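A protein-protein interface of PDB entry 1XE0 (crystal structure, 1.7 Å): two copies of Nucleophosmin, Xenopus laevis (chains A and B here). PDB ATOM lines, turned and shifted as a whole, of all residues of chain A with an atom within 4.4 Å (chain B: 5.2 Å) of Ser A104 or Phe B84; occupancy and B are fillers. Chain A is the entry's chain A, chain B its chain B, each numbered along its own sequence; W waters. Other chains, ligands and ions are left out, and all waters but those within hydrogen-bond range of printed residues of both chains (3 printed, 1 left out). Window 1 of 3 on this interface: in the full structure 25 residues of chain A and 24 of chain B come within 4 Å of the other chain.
Printed residues of chain B within 4 Å of Ser A104: Ile B66, Ala B67 and Phe B84.
Printed residues of chain B within 4 Å of Gln A106: Phe B84 and Glu B85.
Printed residues of chain A within 4 Å of Glu B85: Gln A106.
The nearest printed residue of chain B that does not touch Ser A104 is Leu B68 (4.3 Å).
The nearest printed residue of chain A that does not touch Phe B84 is Thr A38 (4.8 Å).
O of Phe B84 is in hydrogen-bond range of N of Leu B36 (2.9 Å).
N of Phe A10 lies within hydrogen-bond range of O of Gly A105 (2.8 Å).
The backbone carbonyl oxygen of Leu B36 lies within hydrogen-bond range of the backbone NH of Gly B83, at 3.0 Å.
The side-chain hydroxyl (OG1) of Thr A38 is in hydrogen-bond range of the side-chain hydroxyl (OG) of Ser A104, at 2.6 Å.
N of Arg A37 lies within hydrogen-bond range of O of Ser A104, 2.7 Å away.
Among the printed residues, merely in contact across the chains: Phe A10 with Ile B66 (3.7 Å), Arg A37 with Phe B84 (3.5 Å), Thr A38 with Ala B67 (3.9 Å), Thr A38 with Leu B81 (3.5 Å), Tyr A102 with Ala B67 (3.7 Å), Ser A104 with Ile B66 (3.99 Å), Ser A104 with Ala B67 (3.4 Å), Ser A104 with Phe B84 (3.4 Å), Gly A105 with Phe B84 (3.6 Å) and Gln A106 with Phe B84 (3.7 Å).
The side-chain amide oxygen of Gln A106 lies close to the backbone carbonyl oxygen of Glu B85 (3.0 Å).
O of Gly B83 sits at hydrogen-bond distance from NH1 of Arg A37 (3.4 Å).
The guanidinium group of Arg A37 sits at hydrogen-bond distance from the backbone carbonyl oxygen of Leu B81, at 3.0 Å.
NH1 of Arg A37 sits at hydrogen-bond distance from O of Gly B82 (3.4 Å).
The side-chain hydroxyl (OG1) of Thr A38 is in hydrogen-bond range of the backbone carbonyl oxygen (O) of Leu B68 (2.8 Å).
Position printed for both chains: 36.
Printed residues of chain A that touch a printed residue of chain B: Phe A10, Arg A37, Thr A38, Tyr A102, Ser A104, Gly A105 and Gln A106.
Along chain A the printed residues that touch a printed residue of chain B span positions 10 to 106.
Of the 12 printed residues of chain B, 8 touch a printed residue of chain A.
Along chain B the printed residues that touch a printed residue of chain A span positions 66 to 85.
Among the printed residues, no Asp or Glu carboxylate lies within 4 Å of a Lys or Arg side-chain nitrogen of the other chain.
Water W1 lies within hydrogen-bond range of O of Ala B67 (2.6 Å), OG1 of Thr A38 (2.9 Å) and O of Tyr A102 (3.2 Å).
Water W2 lies within hydrogen-bond range of NH2 of Arg A37 (2.8 Å) and O of Gly B82 (3.5 Å).
Water W3 bridges the backbone carbonyl oxygen of Val A103 (2.9 Å) and the backbone NH of Ala B67 (3.2 Å).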
ATOM      1  N   PHE A  10     -26.178 -19.573   3.823  1.00  0.00           N
ATOM      2  CA  PHE A  10     -24.747 -19.491   3.760  1.00  0.00           C
ATOM      3  C   PHE A  10     -24.130 -20.578   4.660  1.00  0.00           C
ATOM      4  O   PHE A  10     -24.643 -20.841   5.775  1.00  0.00           O
ATOM      5  CB  PHE A  10     -24.263 -18.176   4.282  1.00  0.00           C
ATOM      6  CG  PHE A  10     -22.759 -18.177   4.468  1.00  0.00           C
ATOM      7  CD1 PHE A  10     -21.949 -18.116   3.320  1.00  0.00           C
ATOM      8  CD2 PHE A  10     -22.193 -18.517   5.671  1.00  0.00           C
ATOM      9  CE1 PHE A  10     -20.546 -18.200   3.380  1.00  0.00           C
ATOM     10  CE2 PHE A  10     -20.779 -18.606   5.758  1.00  0.00           C
ATOM     11  CZ  PHE A  10     -19.950 -18.440   4.609  1.00  0.00           C
ATOM     12  N   LEU A  36     -24.434 -14.366  10.731  1.00  0.00           N
ATOM     13  CA  LEU A  36     -23.980 -15.666  11.214  1.00  0.00           C
ATOM     14  C   LEU A  36     -24.923 -16.257  12.227  1.00  0.00           C
ATOM     15  O   LEU A  36     -25.379 -15.540  13.177  1.00  0.00           O
ATOM     16  CB  LEU A  36     -22.598 -15.565  11.789  1.00  0.00           C
ATOM     17  CG  LEU A  36     -21.528 -15.187  10.784  1.00  0.00           C
ATOM     18  CD1 LEU A  36     -20.211 -15.206  11.515  1.00  0.00           C
ATOM     19  CD2 LEU A  36     -21.480 -16.115   9.576  1.00  0.00           C
ATOM     20  N   ARG A  37     -25.276 -17.540  12.045  1.00  0.00           N
ATOM     21  CA  ARG A  37     -26.300 -18.135  12.901  1.00  0.00           C
ATOM     22  C   ARG A  37     -25.745 -19.168  13.887  1.00  0.00           C
ATOM     23  O   ARG A  37     -26.055 -19.152  15.046  1.00  0.00           O
ATOM     24  CB  ARG A  37     -27.421 -18.759  12.092  1.00  0.00           C
ATOM     25  CG  ARG A  37     -28.337 -17.764  11.596  1.00  0.00           C
ATOM     26  CD  ARG A  37     -29.256 -17.513  12.837  1.00  0.00           C
ATOM     27  NE  ARG A  37     -29.863 -16.382  12.600  1.00  0.00           N
ATOM     28  CZ  ARG A  37     -30.730 -15.811  13.302  1.00  0.00           C
ATOM     29  NH1 ARG A  37     -31.258 -16.339  14.421  1.00  0.00           N
ATOM     30  NH2 ARG A  37     -31.081 -14.684  12.813  1.00  0.00           N
ATOM     31  N   THR A  38     -24.981 -20.110  13.387  1.00  0.00           N
ATOM     32  CA  THR A  38     -24.406 -21.123  14.223  1.00  0.00           C
ATOM     33  C   THR A  38     -22.973 -21.458  13.842  1.00  0.00           C
ATOM     34  O   THR A  38     -22.570 -21.306  12.690  1.00  0.00           O
ATOM     35  CB  THR A  38     -25.225 -22.377  14.296  1.00  0.00           C
ATOM     36  OG1 THR A  38     -25.089 -23.096  13.070  1.00  0.00           O
ATOM     37  CG2 THR A  38     -26.750 -22.104  14.438  1.00  0.00           C
ATOM     38  N   TYR A 102     -18.202 -26.052  11.342  1.00  0.00           N
ATOM     39  CA  TYR A 102     -19.096 -25.505  10.366  1.00  0.00           C
ATOM     40  C   TYR A 102     -19.626 -24.187  10.846  1.00  0.00           C
ATOM     41  O   TYR A 102     -19.869 -23.985  12.034  1.00  0.00           O
ATOM     42  CB  TYR A 102     -20.258 -26.526  10.126  1.00  0.00           C
ATOM     43  CG  TYR A 102     -19.761 -27.816   9.520  1.00  0.00           C
ATOM     44  CD1 TYR A 102     -19.320 -28.840  10.343  1.00  0.00           C
ATOM     45  CD2 TYR A 102     -19.604 -27.956   8.188  1.00  0.00           C
ATOM     46  CE1 TYR A 102     -18.766 -29.989   9.796  1.00  0.00           C
ATOM     47  CE2 TYR A 102     -19.105 -29.094   7.673  1.00  0.00           C
ATOM     48  CZ  TYR A 102     -18.680 -30.099   8.479  1.00  0.00           C
ATOM     49  OH  TYR A 102     -18.070 -31.279   7.954  1.00  0.00           O
ATOM     50  N   VAL A 103     -19.775 -23.276   9.919  1.00  0.00           N
ATOM     51  CA  VAL A 103     -20.464 -22.071  10.183  1.00  0.00           C
ATOM     52  C   VAL A 103     -21.669 -22.001   9.258  1.00  0.00           C
ATOM     53  O   VAL A 103     -21.611 -22.386   8.082  1.00  0.00           O
ATOM     54  CB  VAL A 103     -19.586 -20.858   9.958  1.00  0.00           C
ATOM     55  CG1 VAL A 103     -20.342 -19.559  10.340  1.00  0.00           C
ATOM     56  CG2 VAL A 103     -18.231 -21.005  10.684  1.00  0.00           C
ATOM     57  N   SER A 104     -22.810 -21.604   9.839  1.00  0.00           N
ATOM     58  CA  SER A 104     -24.068 -21.444   9.121  1.00  0.00           C
ATOM     59  C   SER A 104     -24.599 -20.060   9.267  1.00  0.00           C
ATOM     60  O   SER A 104     -24.349 -19.418  10.269  1.00  0.00           O
ATOM     61  CB  SER A 104     -25.115 -22.461   9.519  1.00  0.00           C
ATOM     62  OG  SER A 104     -25.818 -22.103  10.730  1.00  0.00           O
ATOM     63  N   GLY A 105     -25.321 -19.607   8.249  1.00  0.00           N
ATOM     64  CA  GLY A 105     -26.012 -18.356   8.372  1.00  0.00           C
ATOM     65  C   GLY A 105     -26.767 -17.993   7.137  1.00  0.00           C
ATOM     66  O   GLY A 105     -27.170 -18.830   6.360  1.00  0.00           O
ATOM     67  N   GLN A 106     -26.987 -16.693   6.982  1.00  0.00           N
ATOM     68  CA  GLN A 106     -27.831 -16.137   5.964  1.00  0.00           C
ATOM     69  C   GLN A 106     -27.016 -15.128   5.215  1.00  0.00           C
ATOM     70  O   GLN A 106     -26.225 -14.357   5.779  1.00  0.00           O
ATOM     71  CB  GLN A 106     -29.013 -15.431   6.562  1.00  0.00           C
ATOM     72  CG  GLN A 106     -29.968 -16.284   7.401  1.00  0.00           C
ATOM     73  CD  GLN A 106     -30.842 -15.463   8.245  1.00  0.00           C
ATOM     74  OE1 GLN A 106     -32.011 -15.773   8.454  1.00  0.00           O
ATOM     75  NE2 GLN A 106     -30.313 -14.308   8.649  1.00  0.00           N
ATOM     76  N   LEU B  34     -39.355 -20.282   6.735  1.00  0.00           N
ATOM     77  CA  LEU B  34     -39.311 -21.251   7.831  1.00  0.00           C
ATOM     78  C   LEU B  34     -38.365 -20.639   8.803  1.00  0.00           C
ATOM     79  O   LEU B  34     -37.229 -20.464   8.486  1.00  0.00           O
ATOM     80  CB  LEU B  34     -38.826 -22.585   7.318  1.00  0.00           C
ATOM     81  CG  LEU B  34     -38.616 -23.678   8.332  1.00  0.00           C
ATOM     82  CD1 LEU B  34     -39.911 -24.050   9.072  1.00  0.00           C
ATOM     83  CD2 LEU B  34     -37.928 -24.902   7.824  1.00  0.00           C
ATOM     84  N   SER B  35     -38.807 -20.295  10.026  1.00  0.00           N
ATOM     85  CA  SER B  35     -37.970 -19.723  10.984  1.00  0.00           C
ATOM     86  C   SER B  35     -37.698 -20.816  12.047  1.00  0.00           C
ATOM     87  O   SER B  35     -38.600 -21.214  12.827  1.00  0.00           O
ATOM     88  CB  SER B  35     -38.588 -18.487  11.591  1.00  0.00           C
ATOM     89  OG  SER B  35     -37.784 -18.010  12.619  1.00  0.00           O
ATOM     90  N   LEU B  36     -36.450 -21.270  12.117  1.00  0.00           N
ATOM     91  CA  LEU B  36     -36.078 -22.334  13.037  1.00  0.00           C
ATOM     92  C   LEU B  36     -35.831 -21.806  14.439  1.00  0.00           C
ATOM     93  O   LEU B  36     -35.115 -20.869  14.631  1.00  0.00           O
ATOM     94  CB  LEU B  36     -34.827 -23.065  12.533  1.00  0.00           C
ATOM     95  CG  LEU B  36     -35.013 -23.729  11.124  1.00  0.00           C
ATOM     96  CD1 LEU B  36     -33.785 -24.360  10.753  1.00  0.00           C
ATOM     97  CD2 LEU B  36     -36.123 -24.717  11.055  1.00  0.00           C
ATOM     98  N   ILE B  66     -25.651 -27.091   4.669  1.00  0.00           N
ATOM     99  CA  ILE B  66     -25.002 -26.365   5.742  1.00  0.00           C
ATOM    100  C   ILE B  66     -25.375 -27.059   7.073  1.00  0.00           C
ATOM    101  O   ILE B  66     -26.476 -27.429   7.250  1.00  0.00           O
ATOM    102  CB  ILE B  66     -25.463 -24.891   5.778  1.00  0.00           C
ATOM    103  CG1 ILE B  66     -26.907 -24.738   6.192  1.00  0.00           C
ATOM    104  CG2 ILE B  66     -25.216 -24.224   4.487  1.00  0.00           C
ATOM    105  CD1 ILE B  66     -27.370 -23.278   6.332  1.00  0.00           C
ATOM    106  N   ALA B  67     -24.446 -27.235   7.995  1.00  0.00           N
ATOM    107  CA  ALA B  67     -24.738 -27.853   9.275  1.00  0.00           C
ATOM    108  C   ALA B  67     -25.315 -26.771  10.139  1.00  0.00           C
ATOM    109  O   ALA B  67     -24.682 -25.762  10.271  1.00  0.00           O
ATOM    110  CB  ALA B  67     -23.437 -28.356   9.908  1.00  0.00           C
ATOM    111  N   LEU B  68     -26.455 -27.042  10.751  1.00  0.00           N
ATOM    112  CA  LEU B  68     -27.173 -26.128  11.644  1.00  0.00           C
ATOM    113  C   LEU B  68     -26.772 -26.336  13.068  1.00  0.00           C
ATOM    114  O   LEU B  68     -26.575 -25.322  13.784  1.00  0.00           O
ATOM    115  CB  LEU B  68     -28.675 -26.320  11.547  1.00  0.00           C
ATOM    116  CG  LEU B  68     -29.384 -26.124  10.229  1.00  0.00           C
ATOM    117  CD1 LEU B  68     -30.684 -26.739  10.343  1.00  0.00           C
ATOM    118  CD2 LEU B  68     -29.556 -24.659   9.922  1.00  0.00           C
ATOM    119  N   LEU B  81     -31.839 -21.826  18.049  1.00  0.00           N
ATOM    120  CA  LEU B  81     -31.331 -21.018  16.961  1.00  0.00           C
ATOM    121  C   LEU B  81     -31.873 -19.617  16.865  1.00  0.00           C
ATOM    122  O   LEU B  81     -31.279 -18.781  16.121  1.00  0.00           O
ATOM    123  CB  LEU B  81     -31.656 -21.730  15.626  1.00  0.00           C
ATOM    124  CG  LEU B  81     -31.253 -23.212  15.612  1.00  0.00           C
ATOM    125  CD1 LEU B  81     -31.635 -23.873  14.288  1.00  0.00           C
ATOM    126  CD2 LEU B  81     -29.781 -23.271  15.767  1.00  0.00           C
ATOM    127  N   GLY B  82     -32.932 -19.310  17.646  1.00  0.00           N
ATOM    128  CA  GLY B  82     -33.340 -17.946  17.831  1.00  0.00           C
ATOM    129  C   GLY B  82     -33.998 -17.327  16.580  1.00  0.00           C
ATOM    130  O   GLY B  82     -34.008 -16.106  16.472  1.00  0.00           O
ATOM    131  N   GLY B  83     -34.603 -18.136  15.712  1.00  0.00           N
ATOM    132  CA  GLY B  83     -35.357 -17.648  14.544  1.00  0.00           C
ATOM    133  C   GLY B  83     -34.432 -17.496  13.329  1.00  0.00           C
ATOM    134  O   GLY B  83     -34.285 -16.429  12.774  1.00  0.00           O
ATOM    135  N   PHE B  84     -33.807 -18.584  12.955  1.00  0.00           N
ATOM    136  CA  PHE B  84     -33.027 -18.696  11.727  1.00  0.00           C
ATOM    137  C   PHE B  84     -34.006 -18.920  10.584  1.00  0.00           C
ATOM    138  O   PHE B  84     -34.540 -20.044  10.386  1.00  0.00           O
ATOM    139  CB  PHE B  84     -32.160 -19.940  11.876  1.00  0.00           C
ATOM    140  CG  PHE B  84     -31.118 -20.168  10.765  1.00  0.00           C
ATOM    141  CD1 PHE B  84     -29.977 -20.970  11.022  1.00  0.00           C
ATOM    142  CD2 PHE B  84     -31.237 -19.622   9.560  1.00  0.00           C
ATOM    143  CE1 PHE B  84     -29.003 -21.228   9.999  1.00  0.00           C
ATOM    144  CE2 PHE B  84     -30.197 -19.810   8.545  1.00  0.00           C
ATOM    145  CZ  PHE B  84     -29.126 -20.657   8.802  1.00  0.00           C
ATOM    146  N   GLU B  85     -34.250 -17.857   9.841  1.00  0.00           N
ATOM    147  CA  GLU B  85     -35.197 -17.926   8.718  1.00  0.00           C
ATOM    148  C   GLU B  85     -34.565 -18.461   7.493  1.00  0.00           C
ATOM    149  O   GLU B  85     -33.510 -18.018   7.124  1.00  0.00           O
ATOM    150  CB  GLU B  85     -35.708 -16.497   8.408  1.00  0.00           C
ATOM    151  CG  GLU B  85     -36.425 -15.915   9.603  1.00  0.00           C
ATOM    152  CD  GLU B  85     -37.261 -14.656   9.408  1.00  0.00           C
ATOM    153  OE1 GLU B  85     -37.700 -14.138  10.474  1.00  0.00           O
ATOM    154  OE2 GLU B  85     -37.609 -14.273   8.279  1.00  0.00           O
ATOM    155  N   ILE B  86     -35.240 -19.402   6.868  1.00  0.00           N
ATOM    156  CA  ILE B  86     -34.834 -19.939   5.613  1.00  0.00           C
ATOM    157  C   ILE B  86     -36.001 -19.870   4.607  1.00  0.00           C
ATOM    158  O   ILE B  86     -37.158 -20.159   4.943  1.00  0.00           O
ATOM    159  CB  ILE B  86     -34.396 -21.400   5.758  1.00  0.00           C
ATOM    160  CG1 ILE B  86     -33.323 -21.503   6.808  1.00  0.00           C
ATOM    161  CG2 ILE B  86     -33.957 -21.890   4.359  1.00  0.00           C
ATOM    162  CD1 ILE B  86     -32.830 -22.966   7.214  1.00  0.00           C
HETATM  163  O   HOH W   1     -23.006 -24.782  12.069  1.00  0.00           O
HETATM  164  O   HOH W   2     -32.570 -13.424  14.831  1.00  0.00           O
HETATM  165  O   HOH W   3     -22.135 -25.189   7.347  1.00  0.00           O
